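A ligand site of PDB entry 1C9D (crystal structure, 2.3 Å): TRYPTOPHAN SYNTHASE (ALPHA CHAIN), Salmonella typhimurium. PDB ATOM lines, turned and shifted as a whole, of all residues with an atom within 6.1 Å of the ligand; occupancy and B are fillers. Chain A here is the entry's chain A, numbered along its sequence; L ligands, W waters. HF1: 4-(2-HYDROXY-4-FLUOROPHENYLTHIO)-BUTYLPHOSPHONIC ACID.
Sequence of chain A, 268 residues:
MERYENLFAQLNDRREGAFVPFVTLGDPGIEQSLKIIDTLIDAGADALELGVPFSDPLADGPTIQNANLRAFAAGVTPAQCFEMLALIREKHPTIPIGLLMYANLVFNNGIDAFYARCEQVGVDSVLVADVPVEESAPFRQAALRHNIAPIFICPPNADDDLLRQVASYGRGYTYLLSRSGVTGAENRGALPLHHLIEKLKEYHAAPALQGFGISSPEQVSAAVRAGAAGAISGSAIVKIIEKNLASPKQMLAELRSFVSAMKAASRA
N of Gly 184 is in hydrogen-bond range of O1 of the ligand (3.0 Å). S1 of the ligand sits close to OH of Tyr 175, at 3.6 Å. N of Gly 234 sits at hydrogen-bond distance from O3 of the ligand, 3.0 Å away. An oxygen (O1) of the ligand sits at hydrogen-bond distance from the backbone NH (N) of Gly 213, at 2.9 Å. An oxygen (O2) of the ligand lies within hydrogen-bond range of the backbone NH (N) of Ser 235 (2.8 Å). An oxygen (OH) of the ligand is in hydrogen-bond range of the side-chain carboxylate (OD1) of Asp 60 (2.8 Å). The side-chain hydroxyl (OG) of Ser 235 sits at hydrogen-bond distance from an oxygen (O2) of the ligand, at 2.5 Å.
OG of Ser 233 is in hydrogen-bond range of O of Ile 214 (2.8 Å). The side-chain carboxylate (OD1) of Asp 60 is in hydrogen-bond range of the side-chain hydroxyl (OG1) of Thr 183. O of Gly 184 is in hydrogen-bond range of NH2 of Arg 179 (3.0 Å). The backbone NH (N) of Phe 22 lies within hydrogen-bond range of the backbone carbonyl oxygen (O) of Ser 233 (3.0 Å). The side-chain hydroxyl (OH) of Tyr 102 lies within hydrogen-bond range of the side-chain carboxylate (OD2) of Asp 60, at 2.8 Å. N of Ala 59 lies within hydrogen-bond range of OH of Tyr 102, at 3.2 Å. N of Thr 183 sits at hydrogen-bond distance from O of Ala 59.
Merely in contact with the ligand: Phe 22, Glu 49, Ala 59, Ile 64, Leu 100, Leu 127, Ala 129, Ile 153, Thr 183, Ala 185, Phe 212 and Ser 233. Hydrophobic or aromatic side chains that line the ligand: Phe 22, Ala 59, Ile 64, Leu 100, Leu 127, Ala 129, Ile 153, Tyr 175 and Phe 212. 18 residues have an atom within 4 Å of the ligand: Phe 22, Glu 49, Ala 59, Asp 60, Ile 64, Leu 100, Leu 127, Ala 129, Ile 153, Tyr 175, Thr 183, Gly 184, Ala 185, Phe 212, Gly 213, Ser 233, Gly 234 and Ser 235. The nearest printed residue that does not touch the ligand is Ile 232 (4.01 Å).
Water W1 lies within hydrogen-bond range of O3 of the ligand (2.8 Å), N of Ala 236 (2.9 Å), O of Ile 214 (3.0 Å), OG of Ser 233 (3.2 Å) and N of Ser 235 (3.4 Å).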
ATOM      1  N   PHE A  22     -18.364  31.753 -13.005  1.00  0.00           N
ATOM      2  CA  PHE A  22     -16.995  31.288 -12.799  1.00  0.00           C
ATOM      3  C   PHE A  22     -16.060  32.471 -12.595  1.00  0.00           C
ATOM      4  O   PHE A  22     -16.316  33.568 -13.078  1.00  0.00           O
ATOM      5  CB  PHE A  22     -16.523  30.447 -13.995  1.00  0.00           C
ATOM      6  CG  PHE A  22     -15.033  30.135 -13.989  1.00  0.00           C
ATOM      7  CD1 PHE A  22     -14.114  31.055 -14.503  1.00  0.00           C
ATOM      8  CD2 PHE A  22     -14.551  28.934 -13.490  1.00  0.00           C
ATOM      9  CE1 PHE A  22     -12.752  30.780 -14.506  1.00  0.00           C
ATOM     10  CE2 PHE A  22     -13.186  28.647 -13.488  1.00  0.00           C
ATOM     11  CZ  PHE A  22     -12.289  29.578 -14.004  1.00  0.00           C
ATOM     12  N   GLU A  49     -18.169  27.939  -9.575  1.00  0.00           N
ATOM     13  CA  GLU A  49     -17.136  27.191 -10.306  1.00  0.00           C
ATOM     14  C   GLU A  49     -15.893  28.073 -10.108  1.00  0.00           C
ATOM     15  O   GLU A  49     -15.879  29.239 -10.496  1.00  0.00           O
ATOM     16  CB  GLU A  49     -17.513  27.047 -11.784  1.00  0.00           C
ATOM     17  CG  GLU A  49     -16.813  25.926 -12.573  1.00  0.00           C
ATOM     18  CD  GLU A  49     -16.851  24.543 -11.935  1.00  0.00           C
ATOM     19  OE1 GLU A  49     -17.944  24.065 -11.556  1.00  0.00           O
ATOM     20  OE2 GLU A  49     -15.772  23.924 -11.853  1.00  0.00           O
ATOM     21  N   ALA A  59      -7.186  24.669 -21.932  1.00  0.00           N
ATOM     22  CA  ALA A  59      -8.582  24.539 -22.291  1.00  0.00           C
ATOM     23  C   ALA A  59      -9.259  25.884 -22.146  1.00  0.00           C
ATOM     24  O   ALA A  59     -10.477  25.985 -22.302  1.00  0.00           O
ATOM     25  CB  ALA A  59      -9.265  23.502 -21.428  1.00  0.00           C
ATOM     26  N   ASP A  60      -8.453  26.922 -21.925  1.00  0.00           N
ATOM     27  CA  ASP A  60      -8.977  28.267 -21.728  1.00  0.00           C
ATOM     28  C   ASP A  60      -8.563  29.289 -22.765  1.00  0.00           C
ATOM     29  O   ASP A  60      -7.436  29.274 -23.259  1.00  0.00           O
ATOM     30  CB  ASP A  60      -8.583  28.775 -20.330  1.00  0.00           C
ATOM     31  CG  ASP A  60      -9.340  28.065 -19.209  1.00  0.00           C
ATOM     32  OD1 ASP A  60     -10.596  28.147 -19.208  1.00  0.00           O
ATOM     33  OD2 ASP A  60      -8.693  27.449 -18.341  1.00  0.00           O
ATOM     34  N   ILE A  64      -9.854  34.018 -19.727  1.00  0.00           N
ATOM     35  CA  ILE A  64      -9.517  33.216 -18.550  1.00  0.00           C
ATOM     36  C   ILE A  64      -8.003  33.013 -18.385  1.00  0.00           C
ATOM     37  O   ILE A  64      -7.505  32.898 -17.260  1.00  0.00           O
ATOM     38  CB  ILE A  64     -10.301  31.876 -18.577  1.00  0.00           C
ATOM     39  CG1 ILE A  64     -11.798  32.180 -18.376  1.00  0.00           C
ATOM     40  CG2 ILE A  64      -9.829  30.935 -17.488  1.00  0.00           C
ATOM     41  CD1 ILE A  64     -12.681  30.938 -18.351  1.00  0.00           C
ATOM     42  N   LEU A 100     -12.198  24.036 -10.774  1.00  0.00           N
ATOM     43  CA  LEU A 100     -11.735  23.799 -12.136  1.00  0.00           C
ATOM     44  C   LEU A 100     -10.238  23.591 -11.958  1.00  0.00           C
ATOM     45  O   LEU A 100      -9.528  24.513 -11.551  1.00  0.00           O
ATOM     46  CB  LEU A 100     -12.011  24.990 -13.074  1.00  0.00           C
ATOM     47  CG  LEU A 100     -11.587  24.831 -14.549  1.00  0.00           C
ATOM     48  CD1 LEU A 100     -10.095  25.036 -14.735  1.00  0.00           C
ATOM     49  CD2 LEU A 100     -12.000  23.460 -15.074  1.00  0.00           C
ATOM     50  N   TYR A 102      -6.415  21.389 -13.402  1.00  0.00           N
ATOM     51  CA  TYR A 102      -5.619  20.790 -14.479  1.00  0.00           C
ATOM     52  C   TYR A 102      -4.891  19.642 -13.765  1.00  0.00           C
ATOM     53  O   TYR A 102      -4.620  19.746 -12.565  1.00  0.00           O
ATOM     54  CB  TYR A 102      -4.657  21.783 -15.151  1.00  0.00           C
ATOM     55  CG  TYR A 102      -5.382  22.648 -16.155  1.00  0.00           C
ATOM     56  CD1 TYR A 102      -5.662  22.177 -17.433  1.00  0.00           C
ATOM     57  CD2 TYR A 102      -5.865  23.906 -15.794  1.00  0.00           C
ATOM     58  CE1 TYR A 102      -6.401  22.940 -18.343  1.00  0.00           C
ATOM     59  CE2 TYR A 102      -6.609  24.670 -16.679  1.00  0.00           C
ATOM     60  CZ  TYR A 102      -6.875  24.183 -17.945  1.00  0.00           C
ATOM     61  OH  TYR A 102      -7.588  24.965 -18.820  1.00  0.00           O
ATOM     62  N   LEU A 127     -13.538  19.111 -11.357  1.00  0.00           N
ATOM     63  CA  LEU A 127     -13.421  18.824 -12.778  1.00  0.00           C
ATOM     64  C   LEU A 127     -11.942  19.020 -13.129  1.00  0.00           C
ATOM     65  O   LEU A 127     -11.346  20.052 -12.783  1.00  0.00           O
ATOM     66  CB  LEU A 127     -14.268  19.814 -13.582  1.00  0.00           C
ATOM     67  CG  LEU A 127     -13.966  19.957 -15.085  1.00  0.00           C
ATOM     68  CD1 LEU A 127     -14.136  18.630 -15.804  1.00  0.00           C
ATOM     69  CD2 LEU A 127     -14.868  21.017 -15.683  1.00  0.00           C
ATOM     70  N   ALA A 129      -9.840  19.385 -16.140  1.00  0.00           N
ATOM     71  CA  ALA A 129      -9.982  19.641 -17.570  1.00  0.00           C
ATOM     72  C   ALA A 129      -9.187  18.769 -18.557  1.00  0.00           C
ATOM     73  O   ALA A 129      -9.649  18.550 -19.681  1.00  0.00           O
ATOM     74  CB  ALA A 129      -9.756  21.121 -17.861  1.00  0.00           C
ATOM     75  N   ILE A 153     -17.022  15.360 -18.535  1.00  0.00           N
ATOM     76  CA  ILE A 153     -17.432  16.187 -19.663  1.00  0.00           C
ATOM     77  C   ILE A 153     -18.087  15.400 -20.790  1.00  0.00           C
ATOM     78  O   ILE A 153     -17.582  14.360 -21.213  1.00  0.00           O
ATOM     79  CB  ILE A 153     -16.221  17.020 -20.181  1.00  0.00           C
ATOM     80  CG1 ILE A 153     -16.019  18.232 -19.251  1.00  0.00           C
ATOM     81  CG2 ILE A 153     -16.442  17.475 -21.623  1.00  0.00           C
ATOM     82  CD1 ILE A 153     -14.918  19.176 -19.667  1.00  0.00           C
ATOM     83  N   TYR A 175     -21.173  17.908 -17.063  1.00  0.00           N
ATOM     84  CA  TYR A 175     -20.765  19.118 -17.759  1.00  0.00           C
ATOM     85  C   TYR A 175     -21.072  18.967 -19.245  1.00  0.00           C
ATOM     86  O   TYR A 175     -20.339  18.290 -19.964  1.00  0.00           O
ATOM     87  CB  TYR A 175     -19.264  19.368 -17.542  1.00  0.00           C
ATOM     88  CG  TYR A 175     -18.829  20.814 -17.721  1.00  0.00           C
ATOM     89  CD1 TYR A 175     -18.960  21.464 -18.952  1.00  0.00           C
ATOM     90  CD2 TYR A 175     -18.305  21.548 -16.650  1.00  0.00           C
ATOM     91  CE1 TYR A 175     -18.585  22.788 -19.121  1.00  0.00           C
ATOM     92  CE2 TYR A 175     -17.927  22.886 -16.802  1.00  0.00           C
ATOM     93  CZ  TYR A 175     -18.068  23.499 -18.046  1.00  0.00           C
ATOM     94  OH  TYR A 175     -17.695  24.817 -18.227  1.00  0.00           O
ATOM     95  N   LEU A 177     -20.904  20.225 -22.664  1.00  0.00           N
ATOM     96  CA  LEU A 177     -20.129  21.154 -23.471  1.00  0.00           C
ATOM     97  C   LEU A 177     -21.037  21.566 -24.634  1.00  0.00           C
ATOM     98  O   LEU A 177     -21.509  20.721 -25.398  1.00  0.00           O
ATOM     99  CB  LEU A 177     -18.868  20.435 -23.980  1.00  0.00           C
ATOM    100  CG  LEU A 177     -17.499  21.104 -23.896  1.00  0.00           C
ATOM    101  CD1 LEU A 177     -17.335  21.850 -22.580  1.00  0.00           C
ATOM    102  CD2 LEU A 177     -16.407  20.035 -24.063  1.00  0.00           C
ATOM    103  N   ARG A 179     -20.121  23.678 -27.042  1.00  0.00           N
ATOM    104  CA  ARG A 179     -19.265  23.939 -28.200  1.00  0.00           C
ATOM    105  C   ARG A 179     -18.010  23.079 -28.246  1.00  0.00           C
ATOM    106  O   ARG A 179     -17.701  22.318 -27.333  1.00  0.00           O
ATOM    107  CB  ARG A 179     -18.800  25.397 -28.084  1.00  0.00           C
ATOM    108  CG  ARG A 179     -18.965  26.238 -29.308  1.00  0.00           C
ATOM    109  CD  ARG A 179     -17.941  27.366 -29.290  1.00  0.00           C
ATOM    110  NE  ARG A 179     -17.920  28.147 -28.059  1.00  0.00           N
ATOM    111  CZ  ARG A 179     -16.909  28.159 -27.181  1.00  0.00           C
ATOM    112  NH1 ARG A 179     -15.829  27.406 -27.385  1.00  0.00           N
ATOM    113  NH2 ARG A 179     -16.947  28.957 -26.127  1.00  0.00           N
ATOM    114  N   VAL A 182     -12.096  26.158 -27.083  1.00  0.00           N
ATOM    115  CA  VAL A 182     -11.786  26.531 -25.696  1.00  0.00           C
ATOM    116  C   VAL A 182     -12.783  27.535 -25.093  1.00  0.00           C
ATOM    117  O   VAL A 182     -13.646  28.067 -25.800  1.00  0.00           O
ATOM    118  CB  VAL A 182     -10.337  27.104 -25.560  1.00  0.00           C
ATOM    119  CG1 VAL A 182      -9.336  26.097 -26.044  1.00  0.00           C
ATOM    120  CG2 VAL A 182     -10.198  28.409 -26.330  1.00  0.00           C
ATOM    121  N   THR A 183     -12.657  27.794 -23.796  1.00  0.00           N
ATOM    122  CA  THR A 183     -13.550  28.732 -23.112  1.00  0.00           C
ATOM    123  C   THR A 183     -13.466  30.126 -23.723  1.00  0.00           C
ATOM    124  O   THR A 183     -12.368  30.578 -24.091  1.00  0.00           O
ATOM    125  CB  THR A 183     -13.205  28.862 -21.599  1.00  0.00           C
ATOM    126  OG1 THR A 183     -11.885  29.419 -21.449  1.00  0.00           O
ATOM    127  CG2 THR A 183     -13.253  27.519 -20.898  1.00  0.00           C
ATOM    128  N   GLY A 184     -14.604  30.805 -23.822  1.00  0.00           N
ATOM    129  CA  GLY A 184     -14.619  32.148 -24.386  1.00  0.00           C
ATOM    130  C   GLY A 184     -16.005  32.565 -24.794  1.00  0.00           C
ATOM    131  O   GLY A 184     -16.623  31.925 -25.640  1.00  0.00           O
ATOM    132  N   ALA A 185     -16.516  33.640 -24.190  1.00  0.00           N
ATOM    133  CA  ALA A 185     -17.850  34.169 -24.500  1.00  0.00           C
ATOM    134  C   ALA A 185     -17.792  34.957 -25.809  1.00  0.00           C
ATOM    135  O   ALA A 185     -18.814  35.422 -26.318  1.00  0.00           O
ATOM    136  CB  ALA A 185     -18.339  35.057 -23.369  1.00  0.00           C
ATOM    137  N   GLY A 211     -22.131  24.545 -20.411  1.00  0.00           N
ATOM    138  CA  GLY A 211     -21.052  25.501 -20.287  1.00  0.00           C
ATOM    139  C   GLY A 211     -20.309  25.758 -21.596  1.00  0.00           C
ATOM    140  O   GLY A 211     -20.261  24.856 -22.440  1.00  0.00           O
ATOM    141  N   PHE A 212     -19.714  26.945 -21.695  1.00  0.00           N
ATOM    142  CA  PHE A 212     -18.951  27.439 -22.870  1.00  0.00           C
ATOM    143  C   PHE A 212     -19.797  28.361 -23.746  1.00  0.00           C
ATOM    144  O   PHE A 212     -20.829  27.955 -24.279  1.00  0.00           O
ATOM    145  CB  PHE A 212     -18.379  26.309 -23.743  1.00  0.00           C
ATOM    146  CG  PHE A 212     -17.042  25.761 -23.276  1.00  0.00           C
ATOM    147  CD1 PHE A 212     -16.070  25.393 -24.205  1.00  0.00           C
ATOM    148  CD2 PHE A 212     -16.776  25.547 -21.925  1.00  0.00           C
ATOM    149  CE1 PHE A 212     -14.855  24.806 -23.801  1.00  0.00           C
ATOM    150  CE2 PHE A 212     -15.570  24.965 -21.507  1.00  0.00           C
ATOM    151  CZ  PHE A 212     -14.619  24.590 -22.444  1.00  0.00           C
ATOM    152  N   GLY A 213     -19.371  29.623 -23.841  1.00  0.00           N
ATOM    153  CA  GLY A 213     -20.058  30.609 -24.663  1.00  0.00           C
ATOM    154  C   GLY A 213     -21.344  31.254 -24.156  1.00  0.00           C
ATOM    155  O   GLY A 213     -21.900  32.119 -24.837  1.00  0.00           O
ATOM    156  N   ILE A 214     -21.795  30.871 -22.967  1.00  0.00           N
ATOM    157  CA  ILE A 214     -23.018  31.433 -22.386  1.00  0.00           C
ATOM    158  C   ILE A 214     -22.727  32.830 -21.844  1.00  0.00           C
ATOM    159  O   ILE A 214     -22.055  32.970 -20.824  1.00  0.00           O
ATOM    160  CB  ILE A 214     -23.537  30.532 -21.221  1.00  0.00           C
ATOM    161  CG1 ILE A 214     -23.662  29.067 -21.675  1.00  0.00           C
ATOM    162  CG2 ILE A 214     -24.860  31.077 -20.678  1.00  0.00           C
ATOM    163  CD1 ILE A 214     -24.682  28.815 -22.734  1.00  0.00           C
ATOM    164  N   ILE A 232     -23.518  27.537 -16.950  1.00  0.00           N
ATOM    165  CA  ILE A 232     -22.285  28.100 -16.380  1.00  0.00           C
ATOM    166  C   ILE A 232     -21.784  29.234 -17.294  1.00  0.00           C
ATOM    167  O   ILE A 232     -21.877  29.131 -18.525  1.00  0.00           O
ATOM    168  CB  ILE A 232     -21.186  27.017 -16.268  1.00  0.00           C
ATOM    169  CG1 ILE A 232     -21.654  25.887 -15.339  1.00  0.00           C
ATOM    170  CG2 ILE A 232     -19.876  27.624 -15.754  1.00  0.00           C
ATOM    171  CD1 ILE A 232     -20.857  24.613 -15.473  1.00  0.00           C
ATOM    172  N   SER A 233     -21.251  30.298 -16.700  1.00  0.00           N
ATOM    173  CA  SER A 233     -20.738  31.426 -17.464  1.00  0.00           C
ATOM    174  C   SER A 233     -19.459  31.981 -16.820  1.00  0.00           C
ATOM    175  O   SER A 233     -19.488  32.470 -15.692  1.00  0.00           O
ATOM    176  CB  SER A 233     -21.794  32.533 -17.555  1.00  0.00           C
ATOM    177  OG  SER A 233     -21.303  33.686 -18.216  1.00  0.00           O
ATOM    178  N   GLY A 234     -18.350  31.946 -17.560  1.00  0.00           N
ATOM    179  CA  GLY A 234     -17.072  32.424 -17.046  1.00  0.00           C
ATOM    180  C   GLY A 234     -16.492  33.676 -17.689  1.00  0.00           C
ATOM    181  O   GLY A 234     -16.306  34.687 -17.011  1.00  0.00           O
ATOM    182  N   SER A 235     -16.226  33.633 -18.993  1.00  0.00           N
ATOM    183  CA  SER A 235     -15.649  34.786 -19.685  1.00  0.00           C
ATOM    184  C   SER A 235     -16.452  36.080 -19.519  1.00  0.00           C
ATOM    185  O   SER A 235     -15.875  37.145 -19.255  1.00  0.00           O
ATOM    186  CB  SER A 235     -15.449  34.467 -21.161  1.00  0.00           C
ATOM    187  OG  SER A 235     -14.468  33.449 -21.347  1.00  0.00           O
ATOM    188  N   ALA A 236     -17.770  35.994 -19.637  1.00  0.00           N
ATOM    189  CA  ALA A 236     -18.610  37.179 -19.495  1.00  0.00           C
ATOM    190  C   ALA A 236     -18.452  37.810 -18.102  1.00  0.00           C
ATOM    191  O   ALA A 236     -18.544  39.029 -17.948  1.00  0.00           O
ATOM    192  CB  ALA A 236     -20.072  36.839 -19.756  1.00  0.00           C
HETATM  193  P1  HF1 L   1     -16.867  30.535 -20.911  1.00  0.00           P
HETATM  194  O3  HF1 L   1     -18.071  31.122 -20.424  1.00  0.00           O
HETATM  195  O1  HF1 L   1     -17.039  30.190 -22.264  1.00  0.00           O
HETATM  196  O2  HF1 L   1     -15.809  31.437 -20.759  1.00  0.00           O
HETATM  197  C2  HF1 L   1     -16.233  29.309 -18.452  1.00  0.00           C
HETATM  198  C3  HF1 L   1     -16.124  27.148 -17.100  1.00  0.00           C
HETATM  199  C9  HF1 L   1     -14.367  23.992 -17.793  1.00  0.00           C
HETATM  200  C8  HF1 L   1     -13.959  25.262 -17.286  1.00  0.00           C
HETATM  201  C7  HF1 L   1     -12.713  25.849 -17.724  1.00  0.00           C
HETATM  202  OH  HF1 L   1     -12.259  27.117 -17.239  1.00  0.00           O
HETATM  203  C6  HF1 L   1     -11.894  25.139 -18.631  1.00  0.00           C
HETATM  204  C5  HF1 L   1     -12.309  23.873 -19.124  1.00  0.00           C
HETATM  205  C10 HF1 L   1     -13.557  23.309 -18.687  1.00  0.00           C
HETATM  206  F   HF1 L   1     -13.950  22.079 -19.161  1.00  0.00           F
HETATM  207  S1  HF1 L   1     -15.072  26.058 -16.131  1.00  0.00           S
HETATM  208  C4  HF1 L   1     -15.342  28.351 -17.623  1.00  0.00           C
HETATM  209  C1  HF1 L   1     -16.467  29.016 -19.935  1.00  0.00           C
HETATM  210  O   HOH W   1     -19.180  33.675 -20.577  1.00  0.00           O
HETATM  211  O   HOH W   2     -20.383  29.383 -20.808  1.00  0.00           O
